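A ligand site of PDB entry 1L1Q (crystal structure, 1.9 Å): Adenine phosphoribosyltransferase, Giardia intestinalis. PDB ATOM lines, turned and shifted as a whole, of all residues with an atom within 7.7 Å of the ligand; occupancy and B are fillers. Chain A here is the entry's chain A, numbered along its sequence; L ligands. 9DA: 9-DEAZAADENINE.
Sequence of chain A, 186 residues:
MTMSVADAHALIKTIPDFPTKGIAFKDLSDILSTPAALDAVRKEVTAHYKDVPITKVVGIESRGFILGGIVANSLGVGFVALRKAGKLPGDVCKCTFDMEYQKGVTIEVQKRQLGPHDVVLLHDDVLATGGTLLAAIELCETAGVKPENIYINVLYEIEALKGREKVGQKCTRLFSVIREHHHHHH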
ATOM      1  N   LYS A  13       7.093  13.034  -9.029  1.00  0.00           N
ATOM      2  CA  LYS A  13       5.975  12.736  -9.913  1.00  0.00           C
ATOM      3  C   LYS A  13       6.407  11.636 -10.861  1.00  0.00           C
ATOM      4  O   LYS A  13       7.533  11.628 -11.337  1.00  0.00           O
ATOM      5  CB  LYS A  13       5.568  13.952 -10.746  1.00  0.00           C
ATOM      6  CG  LYS A  13       4.647  14.932 -10.052  1.00  0.00           C
ATOM      7  CD  LYS A  13       5.331  15.633  -8.925  1.00  0.00           C
ATOM      8  CE  LYS A  13       4.486  16.774  -8.382  1.00  0.00           C
ATOM      9  NZ  LYS A  13       5.169  17.367  -7.208  1.00  0.00           N
ATOM     10  N   ILE A  15       5.729  10.158 -14.439  1.00  0.00           N
ATOM     11  CA  ILE A  15       5.147  10.512 -15.734  1.00  0.00           C
ATOM     12  C   ILE A  15       5.126   9.288 -16.654  1.00  0.00           C
ATOM     13  O   ILE A  15       6.187   8.756 -17.008  1.00  0.00           O
ATOM     14  CB  ILE A  15       5.974  11.613 -16.427  1.00  0.00           C
ATOM     15  CG1 ILE A  15       6.231  12.775 -15.450  1.00  0.00           C
ATOM     16  CG2 ILE A  15       5.253  12.099 -17.680  1.00  0.00           C
ATOM     17  CD1 ILE A  15       4.977  13.490 -15.009  1.00  0.00           C
ATOM     18  N   PHE A  18       7.176   8.301 -21.014  1.00  0.00           N
ATOM     19  CA  PHE A  18       8.100   9.405 -21.254  1.00  0.00           C
ATOM     20  C   PHE A  18       9.538   8.968 -20.985  1.00  0.00           C
ATOM     21  O   PHE A  18       9.820   8.352 -19.960  1.00  0.00           O
ATOM     22  CB  PHE A  18       7.777  10.587 -20.361  1.00  0.00           C
ATOM     23  CG  PHE A  18       8.616  11.800 -20.645  1.00  0.00           C
ATOM     24  CD1 PHE A  18       8.252  12.688 -21.653  1.00  0.00           C
ATOM     25  CD2 PHE A  18       9.807  12.023 -19.961  1.00  0.00           C
ATOM     26  CE1 PHE A  18       9.047  13.773 -21.983  1.00  0.00           C
ATOM     27  CE2 PHE A  18      10.622  13.104 -20.283  1.00  0.00           C
ATOM     28  CZ  PHE A  18      10.244  13.984 -21.296  1.00  0.00           C
ATOM     29  N   PRO A  19      10.468   9.290 -21.903  1.00  0.00           N
ATOM     30  CA  PRO A  19      10.264  10.027 -23.152  1.00  0.00           C
ATOM     31  C   PRO A  19       9.557   9.192 -24.231  1.00  0.00           C
ATOM     32  O   PRO A  19       8.859   9.738 -25.081  1.00  0.00           O
ATOM     33  CB  PRO A  19      11.690  10.396 -23.557  1.00  0.00           C
ATOM     34  CG  PRO A  19      12.483   9.211 -23.084  1.00  0.00           C
ATOM     35  CD  PRO A  19      11.893   8.955 -21.709  1.00  0.00           C
ATOM     36  N   ILE A  23       7.863   3.664 -20.775  1.00  0.00           N
ATOM     37  CA  ILE A  23       8.836   4.102 -19.776  1.00  0.00           C
ATOM     38  C   ILE A  23       8.178   4.965 -18.701  1.00  0.00           C
ATOM     39  O   ILE A  23       7.585   5.998 -19.006  1.00  0.00           O
ATOM     40  CB  ILE A  23      10.001   4.919 -20.428  1.00  0.00           C
ATOM     41  CG1 ILE A  23      10.844   4.023 -21.340  1.00  0.00           C
ATOM     42  CG2 ILE A  23      10.882   5.523 -19.342  1.00  0.00           C
ATOM     43  CD1 ILE A  23      10.118   3.514 -22.578  1.00  0.00           C
ATOM     44  N   ALA A  24       8.271   4.533 -17.441  1.00  0.00           N
ATOM     45  CA  ALA A  24       7.712   5.270 -16.318  1.00  0.00           C
ATOM     46  C   ALA A  24       8.790   6.240 -15.813  1.00  0.00           C
ATOM     47  O   ALA A  24       9.678   5.841 -15.064  1.00  0.00           O
ATOM     48  CB  ALA A  24       7.302   4.315 -15.207  1.00  0.00           C
ATOM     49  N   PHE A  25       8.703   7.503 -16.233  1.00  0.00           N
ATOM     50  CA  PHE A  25       9.690   8.523 -15.868  1.00  0.00           C
ATOM     51  C   PHE A  25       9.519   9.138 -14.479  1.00  0.00           C
ATOM     52  O   PHE A  25       8.440   9.599 -14.120  1.00  0.00           O
ATOM     53  CB  PHE A  25       9.682   9.641 -16.914  1.00  0.00           C
ATOM     54  CG  PHE A  25      10.873  10.565 -16.838  1.00  0.00           C
ATOM     55  CD1 PHE A  25      12.053  10.257 -17.520  1.00  0.00           C
ATOM     56  CD2 PHE A  25      10.812  11.732 -16.088  1.00  0.00           C
ATOM     57  CE1 PHE A  25      13.158  11.131 -17.456  1.00  0.00           C
ATOM     58  CE2 PHE A  25      11.914  12.598 -16.021  1.00  0.00           C
ATOM     59  CZ  PHE A  25      13.085  12.293 -16.703  1.00  0.00           C
ATOM     60  N   LYS A  26      10.597   9.165 -13.711  1.00  0.00           N
ATOM     61  CA  LYS A  26      10.571   9.739 -12.363  1.00  0.00           C
ATOM     62  C   LYS A  26      11.046  11.187 -12.434  1.00  0.00           C
ATOM     63  O   LYS A  26      12.237  11.451 -12.627  1.00  0.00           O
ATOM     64  CB  LYS A  26      11.457   8.936 -11.414  1.00  0.00           C
ATOM     65  CG  LYS A  26      11.002   7.504 -11.225  1.00  0.00           C
ATOM     66  CD  LYS A  26       9.628   7.430 -10.575  1.00  0.00           C
ATOM     67  CE  LYS A  26       9.146   5.987 -10.441  1.00  0.00           C
ATOM     68  NZ  LYS A  26       7.826   5.911  -9.767  1.00  0.00           N
ATOM     69  N   ASP A  27      10.101  12.109 -12.282  1.00  0.00           N
ATOM     70  CA  ASP A  27      10.384  13.538 -12.337  1.00  0.00           C
ATOM     71  C   ASP A  27      10.772  14.064 -10.943  1.00  0.00           C
ATOM     72  O   ASP A  27       9.914  14.201 -10.073  1.00  0.00           O
ATOM     73  CB  ASP A  27       9.160  14.292 -12.863  1.00  0.00           C
ATOM     74  CG  ASP A  27       9.437  15.766 -13.102  1.00  0.00           C
ATOM     75  OD1 ASP A  27      10.609  16.151 -12.982  1.00  0.00           O
ATOM     76  OD2 ASP A  27       8.490  16.524 -13.419  1.00  0.00           O
ATOM     77  N   LEU A  28      12.056  14.351 -10.754  1.00  0.00           N
ATOM     78  CA  LEU A  28      12.576  14.834  -9.474  1.00  0.00           C
ATOM     79  C   LEU A  28      12.626  16.347  -9.359  1.00  0.00           C
ATOM     80  O   LEU A  28      13.104  16.897  -8.361  1.00  0.00           O
ATOM     81  CB  LEU A  28      14.000  14.288  -9.262  1.00  0.00           C
ATOM     82  CG  LEU A  28      14.200  12.773  -9.298  1.00  0.00           C
ATOM     83  CD1 LEU A  28      15.655  12.456  -9.030  1.00  0.00           C
ATOM     84  CD2 LEU A  28      13.327  12.116  -8.267  1.00  0.00           C
ATOM     85  N   ARG A  63      22.073  14.843 -15.858  1.00  0.00           N
ATOM     86  CA  ARG A  63      21.095  14.378 -14.885  1.00  0.00           C
ATOM     87  C   ARG A  63      21.653  14.350 -13.461  1.00  0.00           C
ATOM     88  O   ARG A  63      20.912  14.425 -12.482  1.00  0.00           O
ATOM     89  CB  ARG A  63      20.620  12.977 -15.299  1.00  0.00           C
ATOM     90  CG  ARG A  63      21.762  12.016 -15.576  1.00  0.00           C
ATOM     91  CD  ARG A  63      21.323  10.712 -16.231  1.00  0.00           C
ATOM     92  NE  ARG A  63      20.800   9.755 -15.272  1.00  0.00           N
ATOM     93  CZ  ARG A  63      20.795   8.433 -15.469  1.00  0.00           C
ATOM     94  NH1 ARG A  63      21.293   7.937 -16.598  1.00  0.00           N
ATOM     95  NH2 ARG A  63      20.292   7.627 -14.542  1.00  0.00           N
ATOM     96  N   MET A  99      21.494   2.348 -21.392  1.00  0.00           N
ATOM     97  CA  MET A  99      20.638   2.685 -20.248  1.00  0.00           C
ATOM     98  C   MET A  99      19.165   2.367 -20.568  1.00  0.00           C
ATOM     99  O   MET A  99      18.834   2.045 -21.709  1.00  0.00           O
ATOM    100  CB  MET A  99      20.816   4.154 -19.852  1.00  0.00           C
ATOM    101  CG  MET A  99      20.734   5.177 -20.981  1.00  0.00           C
ATOM    102  SD  MET A  99      19.094   5.904 -21.165  1.00  0.00           S
ATOM    103  CE  MET A  99      18.990   6.906 -19.661  1.00  0.00           C
ATOM    104  N   GLU A 100      18.304   2.438 -19.547  1.00  0.00           N
ATOM    105  CA  GLU A 100      16.881   2.104 -19.709  1.00  0.00           C
ATOM    106  C   GLU A 100      16.169   2.485 -21.014  1.00  0.00           C
ATOM    107  O   GLU A 100      15.465   1.658 -21.584  1.00  0.00           O
ATOM    108  CB  GLU A 100      16.066   2.639 -18.521  1.00  0.00           C
ATOM    109  CG  GLU A 100      14.574   2.292 -18.614  1.00  0.00           C
ATOM    110  CD  GLU A 100      13.782   2.698 -17.376  1.00  0.00           C
ATOM    111  OE1 GLU A 100      13.949   3.852 -16.914  1.00  0.00           O
ATOM    112  OE2 GLU A 100      12.983   1.881 -16.868  1.00  0.00           O
ATOM    113  N   TYR A 101      16.329   3.718 -21.485  1.00  0.00           N
ATOM    114  CA  TYR A 101      15.661   4.121 -22.718  1.00  0.00           C
ATOM    115  C   TYR A 101      16.596   4.644 -23.821  1.00  0.00           C
ATOM    116  O   TYR A 101      16.210   5.496 -24.621  1.00  0.00           O
ATOM    117  CB  TYR A 101      14.551   5.134 -22.422  1.00  0.00           C
ATOM    118  CG  TYR A 101      14.977   6.320 -21.586  1.00  0.00           C
ATOM    119  CD1 TYR A 101      15.864   7.269 -22.077  1.00  0.00           C
ATOM    120  CD2 TYR A 101      14.471   6.502 -20.297  1.00  0.00           C
ATOM    121  CE1 TYR A 101      16.253   8.371 -21.314  1.00  0.00           C
ATOM    122  CE2 TYR A 101      14.851   7.606 -19.511  1.00  0.00           C
ATOM    123  CZ  TYR A 101      15.739   8.533 -20.028  1.00  0.00           C
ATOM    124  OH  TYR A 101      16.113   9.625 -19.280  1.00  0.00           O
ATOM    125  N   ASP A 124      24.470   9.924  -9.217  1.00  0.00           N
ATOM    126  CA  ASP A 124      23.515   9.869 -10.305  1.00  0.00           C
ATOM    127  C   ASP A 124      22.136  10.175  -9.717  1.00  0.00           C
ATOM    128  O   ASP A 124      21.866   9.864  -8.556  1.00  0.00           O
ATOM    129  CB  ASP A 124      23.555   8.495 -10.960  1.00  0.00           C
ATOM    130  CG  ASP A 124      23.037   8.516 -12.388  1.00  0.00           C
ATOM    131  OD1 ASP A 124      23.248   9.544 -13.086  1.00  0.00           O
ATOM    132  OD2 ASP A 124      22.448   7.491 -12.815  1.00  0.00           O
ATOM    133  N   ASP A 125      21.277  10.801 -10.504  1.00  0.00           N
ATOM    134  CA  ASP A 125      19.960  11.156 -10.018  1.00  0.00           C
ATOM    135  C   ASP A 125      19.081   9.927  -9.786  1.00  0.00           C
ATOM    136  O   ASP A 125      18.469   9.788  -8.746  1.00  0.00           O
ATOM    137  CB  ASP A 125      19.277  12.134 -10.983  1.00  0.00           C
ATOM    138  CG  ASP A 125      18.893  11.485 -12.305  1.00  0.00           C
ATOM    139  OD1 ASP A 125      17.925  11.973 -12.943  1.00  0.00           O
ATOM    140  OD2 ASP A 125      19.551  10.512 -12.735  1.00  0.00           O
ATOM    141  N   VAL A 126      19.049   9.041 -10.764  1.00  0.00           N
ATOM    142  CA  VAL A 126      18.203   7.844 -10.676  1.00  0.00           C
ATOM    143  C   VAL A 126      18.942   6.572 -11.050  1.00  0.00           C
ATOM    144  O   VAL A 126      19.667   6.535 -12.039  1.00  0.00           O
ATOM    145  CB  VAL A 126      16.992   7.976 -11.646  1.00  0.00           C
ATOM    146  CG1 VAL A 126      16.183   6.664 -11.664  1.00  0.00           C
ATOM    147  CG2 VAL A 126      16.110   9.138 -11.234  1.00  0.00           C
ATOM    148  N   LEU A 127      18.771   5.528 -10.236  1.00  0.00           N
ATOM    149  CA  LEU A 127      19.382   4.230 -10.517  1.00  0.00           C
ATOM    150  C   LEU A 127      18.275   3.348 -11.090  1.00  0.00           C
ATOM    151  O   LEU A 127      17.332   2.979 -10.389  1.00  0.00           O
ATOM    152  CB  LEU A 127      19.950   3.586  -9.240  1.00  0.00           C
ATOM    153  CG  LEU A 127      20.379   2.101  -9.312  1.00  0.00           C
ATOM    154  CD1 LEU A 127      21.314   1.852 -10.499  1.00  0.00           C
ATOM    155  CD2 LEU A 127      21.054   1.684  -8.022  1.00  0.00           C
ATOM    156  N   ALA A 128      18.385   3.050 -12.384  1.00  0.00           N
ATOM    157  CA  ALA A 128      17.404   2.214 -13.057  1.00  0.00           C
ATOM    158  C   ALA A 128      18.032   0.851 -13.340  1.00  0.00           C
ATOM    159  O   ALA A 128      18.111   0.014 -12.443  1.00  0.00           O
ATOM    160  CB  ALA A 128      16.942   2.879 -14.347  1.00  0.00           C
ATOM    161  N   THR A 129      18.480   0.633 -14.576  1.00  0.00           N
ATOM    162  CA  THR A 129      19.095  -0.652 -14.937  1.00  0.00           C
ATOM    163  C   THR A 129      20.523  -0.736 -14.401  1.00  0.00           C
ATOM    164  O   THR A 129      21.054  -1.835 -14.213  1.00  0.00           O
ATOM    165  CB  THR A 129      19.141  -0.860 -16.475  1.00  0.00           C
ATOM    166  OG1 THR A 129      20.067   0.059 -17.058  1.00  0.00           O
ATOM    167  CG2 THR A 129      17.779  -0.639 -17.088  1.00  0.00           C
ATOM    168  N   THR A 132      24.389   2.784 -16.817  1.00  0.00           N
ATOM    169  CA  THR A 132      25.159   4.026 -16.812  1.00  0.00           C
ATOM    170  C   THR A 132      26.180   4.028 -15.675  1.00  0.00           C
ATOM    171  O   THR A 132      27.329   4.426 -15.864  1.00  0.00           O
ATOM    172  CB  THR A 132      24.233   5.252 -16.659  1.00  0.00           C
ATOM    173  OG1 THR A 132      23.218   5.232 -17.663  1.00  0.00           O
ATOM    174  CG2 THR A 132      25.028   6.536 -16.811  1.00  0.00           C
ATOM    175  N   TYR A 156      17.428   8.737  -6.222  1.00  0.00           N
ATOM    176  CA  TYR A 156      16.263   7.847  -6.271  1.00  0.00           C
ATOM    177  C   TYR A 156      16.587   6.473  -6.865  1.00  0.00           C
ATOM    178  O   TYR A 156      17.129   6.395  -7.971  1.00  0.00           O
ATOM    179  CB  TYR A 156      15.180   8.537  -7.097  1.00  0.00           C
ATOM    180  CG  TYR A 156      13.848   7.842  -7.120  1.00  0.00           C
ATOM    181  CD1 TYR A 156      12.887   8.093  -6.155  1.00  0.00           C
ATOM    182  CD2 TYR A 156      13.524   6.962  -8.150  1.00  0.00           C
ATOM    183  CE1 TYR A 156      11.614   7.488  -6.207  1.00  0.00           C
ATOM    184  CE2 TYR A 156      12.268   6.347  -8.212  1.00  0.00           C
ATOM    185  CZ  TYR A 156      11.316   6.618  -7.244  1.00  0.00           C
ATOM    186  OH  TYR A 156      10.074   6.037  -7.321  1.00  0.00           O
ATOM    187  N   ILE A 158      15.110   2.776  -8.195  1.00  0.00           N
ATOM    188  CA  ILE A 158      13.958   1.986  -8.643  1.00  0.00           C
ATOM    189  C   ILE A 158      14.368   0.522  -8.452  1.00  0.00           C
ATOM    190  O   ILE A 158      14.763  -0.147  -9.400  1.00  0.00           O
ATOM    191  CB  ILE A 158      13.647   2.244 -10.130  1.00  0.00           C
ATOM    192  CG1 ILE A 158      13.373   3.725 -10.369  1.00  0.00           C
ATOM    193  CG2 ILE A 158      12.436   1.418 -10.556  1.00  0.00           C
ATOM    194  CD1 ILE A 158      13.221   4.103 -11.826  1.00  0.00           C
ATOM    195  N   LEU A 161      14.083  -2.766 -10.878  1.00  0.00           N
ATOM    196  CA  LEU A 161      14.973  -3.072 -11.995  1.00  0.00           C
ATOM    197  C   LEU A 161      16.294  -3.694 -11.561  1.00  0.00           C
ATOM    198  O   LEU A 161      17.191  -3.869 -12.371  1.00  0.00           O
ATOM    199  CB  LEU A 161      15.236  -1.812 -12.812  1.00  0.00           C
ATOM    200  CG  LEU A 161      14.012  -1.059 -13.338  1.00  0.00           C
ATOM    201  CD1 LEU A 161      14.452   0.206 -14.045  1.00  0.00           C
ATOM    202  CD2 LEU A 161      13.209  -1.947 -14.277  1.00  0.00           C
HETATM  203  N1  9DA L   1      13.107   7.978 -14.674  1.00  0.00           N
HETATM  204  C2  9DA L   1      13.882   9.124 -14.531  1.00  0.00           C
HETATM  205  N3  9DA L   1      15.156   9.183 -14.947  1.00  0.00           N
HETATM  206  C4  9DA L   1      15.587   8.012 -15.530  1.00  0.00           C
HETATM  207  C5  9DA L   1      14.875   6.838 -15.706  1.00  0.00           C
HETATM  208  C6  9DA L   1      13.520   6.766 -15.262  1.00  0.00           C
HETATM  209  N6  9DA L   1      12.702   5.823 -15.317  1.00  0.00           N
HETATM  210  N7  9DA L   1      15.693   5.919 -16.328  1.00  0.00           N
HETATM  211  C8  9DA L   1      16.883   6.518 -16.517  1.00  0.00           C
HETATM  212  C9  9DA L   1      16.870   7.810 -16.041  1.00  0.00           C
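The side-chain carboxylate of Glu 100 is in hydrogen-bond range of a nitrogen (N7) of the ligand, at 2.8 Å.
The backbone NH (N) of Lys 26 is in hydrogen-bond range of a nitrogen (N1) of the ligand (2.9 Å).
O of Ala 24 lies within hydrogen-bond range of N6 of the ligand (3.0 Å).
OH of Tyr 156 sits close to NZ of Lys 26 (3.3 Å).
O of Phe 25 sits at hydrogen-bond distance from N of Ile 15 (2.8 Å).
The backbone NH (N) of Tyr 101 lies close to the side-chain sulfur (SD) of Met 99 (3.5 Å).
NH2 of Arg 63 lies within hydrogen-bond range of O of Val 126, at 2.8 Å.
NE of Arg 63 is in salt-bridge range of OD2 of Asp 125, at 2.9 Å.
The guanidinium group (NH2) of Arg 63 lies within salt-bridge range of the side-chain carboxylate (OD2) of Asp 124, 2.8 Å away.
NH1 of Arg 63 is in hydrogen-bond range of OG1 of Thr 132, at 3.5 Å.
N of Ile 158 sits at hydrogen-bond distance from O of Leu 127.
Merely in contact with the ligand: Phe 25 (3.6 Å), Tyr 101 (3.7 Å), Arg 63 (3.7 Å), Met 99 (3.8 Å), Val 126 (3.8 Å), Ala 128 (3.8 Å) and Ile 158 (3.9 Å).
Of the 24 residues printed, 10 come within 4 Å of the ligand.
Along chain A the residues within 4 Å of the ligand span positions 24 to 158.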
